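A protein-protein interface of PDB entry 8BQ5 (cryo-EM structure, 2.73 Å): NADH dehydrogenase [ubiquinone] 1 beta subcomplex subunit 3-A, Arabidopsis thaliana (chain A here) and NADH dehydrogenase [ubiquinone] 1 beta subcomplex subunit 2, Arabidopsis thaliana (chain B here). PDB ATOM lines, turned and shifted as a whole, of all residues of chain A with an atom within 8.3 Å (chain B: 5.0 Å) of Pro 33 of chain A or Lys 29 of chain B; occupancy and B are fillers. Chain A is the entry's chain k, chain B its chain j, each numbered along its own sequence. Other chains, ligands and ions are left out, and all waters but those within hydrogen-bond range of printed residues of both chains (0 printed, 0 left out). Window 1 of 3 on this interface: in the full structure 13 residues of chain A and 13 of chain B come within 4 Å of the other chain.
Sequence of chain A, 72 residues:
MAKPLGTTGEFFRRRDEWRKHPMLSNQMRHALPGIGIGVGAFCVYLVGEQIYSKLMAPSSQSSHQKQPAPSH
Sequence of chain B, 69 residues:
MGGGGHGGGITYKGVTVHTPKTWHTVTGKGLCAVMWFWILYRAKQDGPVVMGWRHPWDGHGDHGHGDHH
Leu 32 of chain A touches Trp 36 of chain B (CD2 to CZ2, 3.6 Å).
Pro 33 of chain A touches Lys 29 of chain B.
Pro 33 of chain A touches Cys 32 of chain B (O to CB, 3.2 Å).
Gly 34 of chain A touches Lys 29 of chain B.
Gly 34 of chain A touches Ala 33 of chain B (O to CB, 3.4 Å).
Gly 34 of chain A touches Trp 36 of chain B (O to CD1, 3.4 Å).
Ile 35 of chain A touches Trp 36 of chain B (CA to CD1, 3.7 Å).
Gly 38 of chain A touches Ala 33 of chain B.
NE1 of Trp 36 of chain B sits at hydrogen-bond distance from O of Pro 33 of chain A (3.0 Å).
The backbone carbonyl oxygen of Cys 32 of chain B sits close to the indole nitrogen of Trp 36 of chain B, at 3.5 Å.
The side-chain sulfur (SG) of Cys 32 of chain B lies close to the backbone carbonyl oxygen (O) of Gly 28 of chain B.
Of the 10 printed residues of chain A, 5 touch a printed residue of chain B.
Of the 10 printed residues of chain B, 4 touch a printed residue of chain A.
Hydrophobic or aromatic side chains of chain B that line the printed part of chain A: Ala 33 and Trp 36.
Among the printed residues, no Asp or Glu carboxylate lies within 4 Å of a Lys or Arg side-chain nitrogen of the other chain.
Printed residues of chain B within 4 Å of Leu 32 of chain A: Trp 36.
Pro 33 of chain A touches just these residues of chain B: Lys 29 (3.5 Å), Cys 32 (3.2 Å) and Trp 36 (3.0 Å).
Printed residues of chain B within 4 Å of Ile 35 of chain A: Trp 36 (3.7 Å).
No residue of chain A comes within 4 Å of Gly 28 of chain B.
Lys 29 of chain B touches just these residues of chain A: Pro 33 and Gly 34.
No residue of chain A comes within 4 Å of Gly 30 of chain B.
Leu 31 of chain B touches none of the printed residues of chain A.
The nearest printed residue of chain B that does not touch Leu 32 of chain A is Lys 29 of chain B (5.6 Å).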
ATOM      1  N   ARG A  29      22.325  20.362  -1.966  1.00  0.00           N
ATOM      2  CA  ARG A  29      22.785  19.669  -0.729  1.00  0.00           C
ATOM      3  C   ARG A  29      22.622  18.162  -0.952  1.00  0.00           C
ATOM      4  O   ARG A  29      22.971  17.396  -0.030  1.00  0.00           O
ATOM      5  CB  ARG A  29      22.070  20.189   0.526  1.00  0.00           C
ATOM      6  CG  ARG A  29      22.510  19.540   1.830  1.00  0.00           C
ATOM      7  CD  ARG A  29      21.853  20.106   3.071  1.00  0.00           C
ATOM      8  NE  ARG A  29      20.420  19.848   3.075  1.00  0.00           N
ATOM      9  CZ  ARG A  29      19.854  18.717   3.476  1.00  0.00           C
ATOM     10  NH1 ARG A  29      20.601  17.720   3.920  1.00  0.00           N
ATOM     11  NH2 ARG A  29      18.540  18.587   3.435  1.00  0.00           N
ATOM     12  N   HIS A  30      22.120  17.753  -2.121  1.00  0.00           N
ATOM     13  CA  HIS A  30      22.042  16.308  -2.477  1.00  0.00           C
ATOM     14  C   HIS A  30      23.192  15.984  -3.426  1.00  0.00           C
ATOM     15  O   HIS A  30      23.162  14.894  -4.025  1.00  0.00           O
ATOM     16  CB  HIS A  30      20.685  15.979  -3.096  1.00  0.00           C
ATOM     17  CG  HIS A  30      19.529  16.391  -2.249  1.00  0.00           C
ATOM     18  ND1 HIS A  30      18.989  17.661  -2.301  1.00  0.00           N
ATOM     19  CD2 HIS A  30      18.811  15.711  -1.331  1.00  0.00           C
ATOM     20  CE1 HIS A  30      17.992  17.746  -1.446  1.00  0.00           C
ATOM     21  NE2 HIS A  30      17.860  16.562  -0.843  1.00  0.00           N
ATOM     22  N   ALA A  31      24.167  16.891  -3.543  1.00  0.00           N
ATOM     23  CA  ALA A  31      25.290  16.723  -4.494  1.00  0.00           C
ATOM     24  C   ALA A  31      26.097  15.451  -4.228  1.00  0.00           C
ATOM     25  O   ALA A  31      26.640  14.920  -5.198  1.00  0.00           O
ATOM     26  CB  ALA A  31      26.184  17.939  -4.421  1.00  0.00           C
ATOM     27  N   LEU A  32      26.181  14.974  -2.982  1.00  0.00           N
ATOM     28  CA  LEU A  32      27.053  13.843  -2.671  1.00  0.00           C
ATOM     29  C   LEU A  32      26.278  12.795  -1.880  1.00  0.00           C
ATOM     30  O   LEU A  32      26.346  12.754  -0.645  1.00  0.00           O
ATOM     31  CB  LEU A  32      28.293  14.293  -1.903  1.00  0.00           C
ATOM     32  CG  LEU A  32      29.130  15.386  -2.571  1.00  0.00           C
ATOM     33  CD1 LEU A  32      30.212  15.887  -1.629  1.00  0.00           C
ATOM     34  CD2 LEU A  32      29.733  14.891  -3.875  1.00  0.00           C
ATOM     35  N   PRO A  33      25.525  11.937  -2.564  1.00  0.00           N
ATOM     36  CA  PRO A  33      24.872  10.821  -1.871  1.00  0.00           C
ATOM     37  C   PRO A  33      25.895   9.895  -1.233  1.00  0.00           C
ATOM     38  O   PRO A  33      26.981   9.672  -1.773  1.00  0.00           O
ATOM     39  CB  PRO A  33      24.096  10.109  -2.984  1.00  0.00           C
ATOM     40  CG  PRO A  33      24.723  10.569  -4.258  1.00  0.00           C
ATOM     41  CD  PRO A  33      25.236  11.947  -4.006  1.00  0.00           C
ATOM     42  N   GLY A  34      25.539   9.362  -0.066  1.00  0.00           N
ATOM     43  CA  GLY A  34      26.373   8.391   0.612  1.00  0.00           C
ATOM     44  C   GLY A  34      27.721   8.890   1.079  1.00  0.00           C
ATOM     45  O   GLY A  34      28.590   8.068   1.386  1.00  0.00           O
ATOM     46  N   ILE A  35      27.935  10.206   1.137  1.00  0.00           N
ATOM     47  CA  ILE A  35      29.219  10.716   1.610  1.00  0.00           C
ATOM     48  C   ILE A  35      29.389  10.456   3.103  1.00  0.00           C
ATOM     49  O   ILE A  35      30.483  10.098   3.555  1.00  0.00           O
ATOM     50  CB  ILE A  35      29.366  12.212   1.258  1.00  0.00           C
ATOM     51  CG1 ILE A  35      30.768  12.725   1.612  1.00  0.00           C
ATOM     52  CG2 ILE A  35      28.284  13.053   1.923  1.00  0.00           C
ATOM     53  CD1 ILE A  35      31.857  12.287   0.653  1.00  0.00           C
ATOM     54  N   GLY A  36      28.326  10.619   3.888  1.00  0.00           N
ATOM     55  CA  GLY A  36      28.376  10.335   5.308  1.00  0.00           C
ATOM     56  C   GLY A  36      28.568   8.862   5.601  1.00  0.00           C
ATOM     57  O   GLY A  36      29.339   8.492   6.491  1.00  0.00           O
ATOM     58  N   ILE A  37      27.858   8.011   4.860  1.00  0.00           N
ATOM     59  CA  ILE A  37      28.002   6.569   5.038  1.00  0.00           C
ATOM     60  C   ILE A  37      29.416   6.130   4.686  1.00  0.00           C
ATOM     61  O   ILE A  37      30.032   5.331   5.403  1.00  0.00           O
ATOM     62  CB  ILE A  37      26.955   5.818   4.195  1.00  0.00           C
ATOM     63  CG1 ILE A  37      25.675   6.645   4.061  1.00  0.00           C
ATOM     64  CG2 ILE A  37      26.669   4.453   4.801  1.00  0.00           C
ATOM     65  CD1 ILE A  37      24.858   6.733   5.335  1.00  0.00           C
ATOM     66  N   GLY A  38      29.952   6.644   3.577  1.00  0.00           N
ATOM     67  CA  GLY A  38      31.270   6.219   3.135  1.00  0.00           C
ATOM     68  C   GLY A  38      32.380   6.672   4.062  1.00  0.00           C
ATOM     69  O   GLY A  38      33.347   5.940   4.291  1.00  0.00           O
ATOM     70  N   THR B  25      16.401   4.874  -3.893  1.00  0.00           N
ATOM     71  CA  THR B  25      17.155   5.745  -2.998  1.00  0.00           C
ATOM     72  C   THR B  25      18.284   4.977  -2.323  1.00  0.00           C
ATOM     73  O   THR B  25      19.401   5.488  -2.180  1.00  0.00           O
ATOM     74  CB  THR B  25      16.223   6.358  -1.952  1.00  0.00           C
ATOM     75  OG1 THR B  25      15.173   7.078  -2.608  1.00  0.00           O
ATOM     76  CG2 THR B  25      16.990   7.308  -1.046  1.00  0.00           C
ATOM     77  N   VAL B  26      18.006   3.742  -1.900  1.00  0.00           N
ATOM     78  CA  VAL B  26      19.010   2.944  -1.203  1.00  0.00           C
ATOM     79  C   VAL B  26      20.179   2.623  -2.124  1.00  0.00           C
ATOM     80  O   VAL B  26      21.345   2.825  -1.765  1.00  0.00           O
ATOM     81  CB  VAL B  26      18.369   1.663  -0.635  1.00  0.00           C
ATOM     82  CG1 VAL B  26      19.436   0.624  -0.315  1.00  0.00           C
ATOM     83  CG2 VAL B  26      17.546   1.988   0.600  1.00  0.00           C
ATOM     84  N   THR B  27      19.886   2.130  -3.329  1.00  0.00           N
ATOM     85  CA  THR B  27      20.954   1.730  -4.240  1.00  0.00           C
ATOM     86  C   THR B  27      21.822   2.920  -4.626  1.00  0.00           C
ATOM     87  O   THR B  27      23.053   2.807  -4.675  1.00  0.00           O
ATOM     88  CB  THR B  27      20.363   1.070  -5.485  1.00  0.00           C
ATOM     89  OG1 THR B  27      19.136   1.722  -5.832  1.00  0.00           O
ATOM     90  CG2 THR B  27      20.087  -0.400  -5.219  1.00  0.00           C
ATOM     91  N   GLY B  28      21.203   4.066  -4.895  1.00  0.00           N
ATOM     92  CA  GLY B  28      21.942   5.265  -5.237  1.00  0.00           C
ATOM     93  C   GLY B  28      22.858   5.724  -4.123  1.00  0.00           C
ATOM     94  O   GLY B  28      24.014   6.082  -4.364  1.00  0.00           O
ATOM     95  N   LYS B  29      22.347   5.715  -2.890  1.00  0.00           N
ATOM     96  CA  LYS B  29      23.169   6.072  -1.740  1.00  0.00           C
ATOM     97  C   LYS B  29      24.300   5.072  -1.541  1.00  0.00           C
ATOM     98  O   LYS B  29      25.455   5.454  -1.324  1.00  0.00           O
ATOM     99  CB  LYS B  29      22.299   6.151  -0.485  1.00  0.00           C
ATOM    100  CG  LYS B  29      21.494   7.429  -0.365  1.00  0.00           C
ATOM    101  CD  LYS B  29      22.257   8.483   0.411  1.00  0.00           C
ATOM    102  CE  LYS B  29      21.502   9.800   0.440  1.00  0.00           C
ATOM    103  NZ  LYS B  29      21.260  10.325  -0.932  1.00  0.00           N
ATOM    104  N   GLY B  30      23.981   3.779  -1.611  1.00  0.00           N
ATOM    105  CA  GLY B  30      24.979   2.763  -1.320  1.00  0.00           C
ATOM    106  C   GLY B  30      26.121   2.739  -2.317  1.00  0.00           C
ATOM    107  O   GLY B  30      27.291   2.697  -1.930  1.00  0.00           O
ATOM    108  N   LEU B  31      25.799   2.777  -3.613  1.00  0.00           N
ATOM    109  CA  LEU B  31      26.833   2.656  -4.638  1.00  0.00           C
ATOM    110  C   LEU B  31      27.800   3.830  -4.593  1.00  0.00           C
ATOM    111  O   LEU B  31      29.013   3.651  -4.752  1.00  0.00           O
ATOM    112  CB  LEU B  31      26.195   2.536  -6.022  1.00  0.00           C
ATOM    113  CG  LEU B  31      25.960   1.120  -6.557  1.00  0.00           C
ATOM    114  CD1 LEU B  31      25.484   0.170  -5.464  1.00  0.00           C
ATOM    115  CD2 LEU B  31      24.974   1.145  -7.710  1.00  0.00           C
ATOM    116  N   CYS B  32      27.283   5.043  -4.389  1.00  0.00           N
ATOM    117  CA  CYS B  32      28.172   6.182  -4.195  1.00  0.00           C
ATOM    118  C   CYS B  32      29.011   6.014  -2.936  1.00  0.00           C
ATOM    119  O   CYS B  32      30.205   6.337  -2.940  1.00  0.00           O
ATOM    120  CB  CYS B  32      27.368   7.479  -4.138  1.00  0.00           C
ATOM    121  SG  CYS B  32      26.865   8.110  -5.755  1.00  0.00           S
ATOM    122  N   ALA B  33      28.413   5.493  -1.861  1.00  0.00           N
ATOM    123  CA  ALA B  33      29.152   5.289  -0.619  1.00  0.00           C
ATOM    124  C   ALA B  33      30.304   4.309  -0.807  1.00  0.00           C
ATOM    125  O   ALA B  33      31.401   4.529  -0.281  1.00  0.00           O
ATOM    126  CB  ALA B  33      28.209   4.802   0.480  1.00  0.00           C
ATOM    127  N   TRP B  36      33.029   6.280  -2.439  1.00  0.00           N
ATOM    128  CA  TRP B  36      33.773   7.134  -1.516  1.00  0.00           C
ATOM    129  C   TRP B  36      34.721   6.311  -0.656  1.00  0.00           C
ATOM    130  O   TRP B  36      35.885   6.683  -0.469  1.00  0.00           O
ATOM    131  CB  TRP B  36      32.813   7.931  -0.629  1.00  0.00           C
ATOM    132  CG  TRP B  36      31.841   8.794  -1.375  1.00  0.00           C
ATOM    133  CD1 TRP B  36      30.482   8.735  -1.311  1.00  0.00           C
ATOM    134  CD2 TRP B  36      32.154   9.857  -2.283  1.00  0.00           C
ATOM    135  NE1 TRP B  36      29.925   9.684  -2.130  1.00  0.00           N
ATOM    136  CE2 TRP B  36      30.930  10.389  -2.737  1.00  0.00           C
ATOM    137  CE3 TRP B  36      33.347  10.409  -2.759  1.00  0.00           C
ATOM    138  CZ2 TRP B  36      30.866  11.445  -3.643  1.00  0.00           C
ATOM    139  CZ3 TRP B  36      33.281  11.455  -3.659  1.00  0.00           C
ATOM    140  CH2 TRP B  36      32.049  11.962  -4.090  1.00  0.00           C
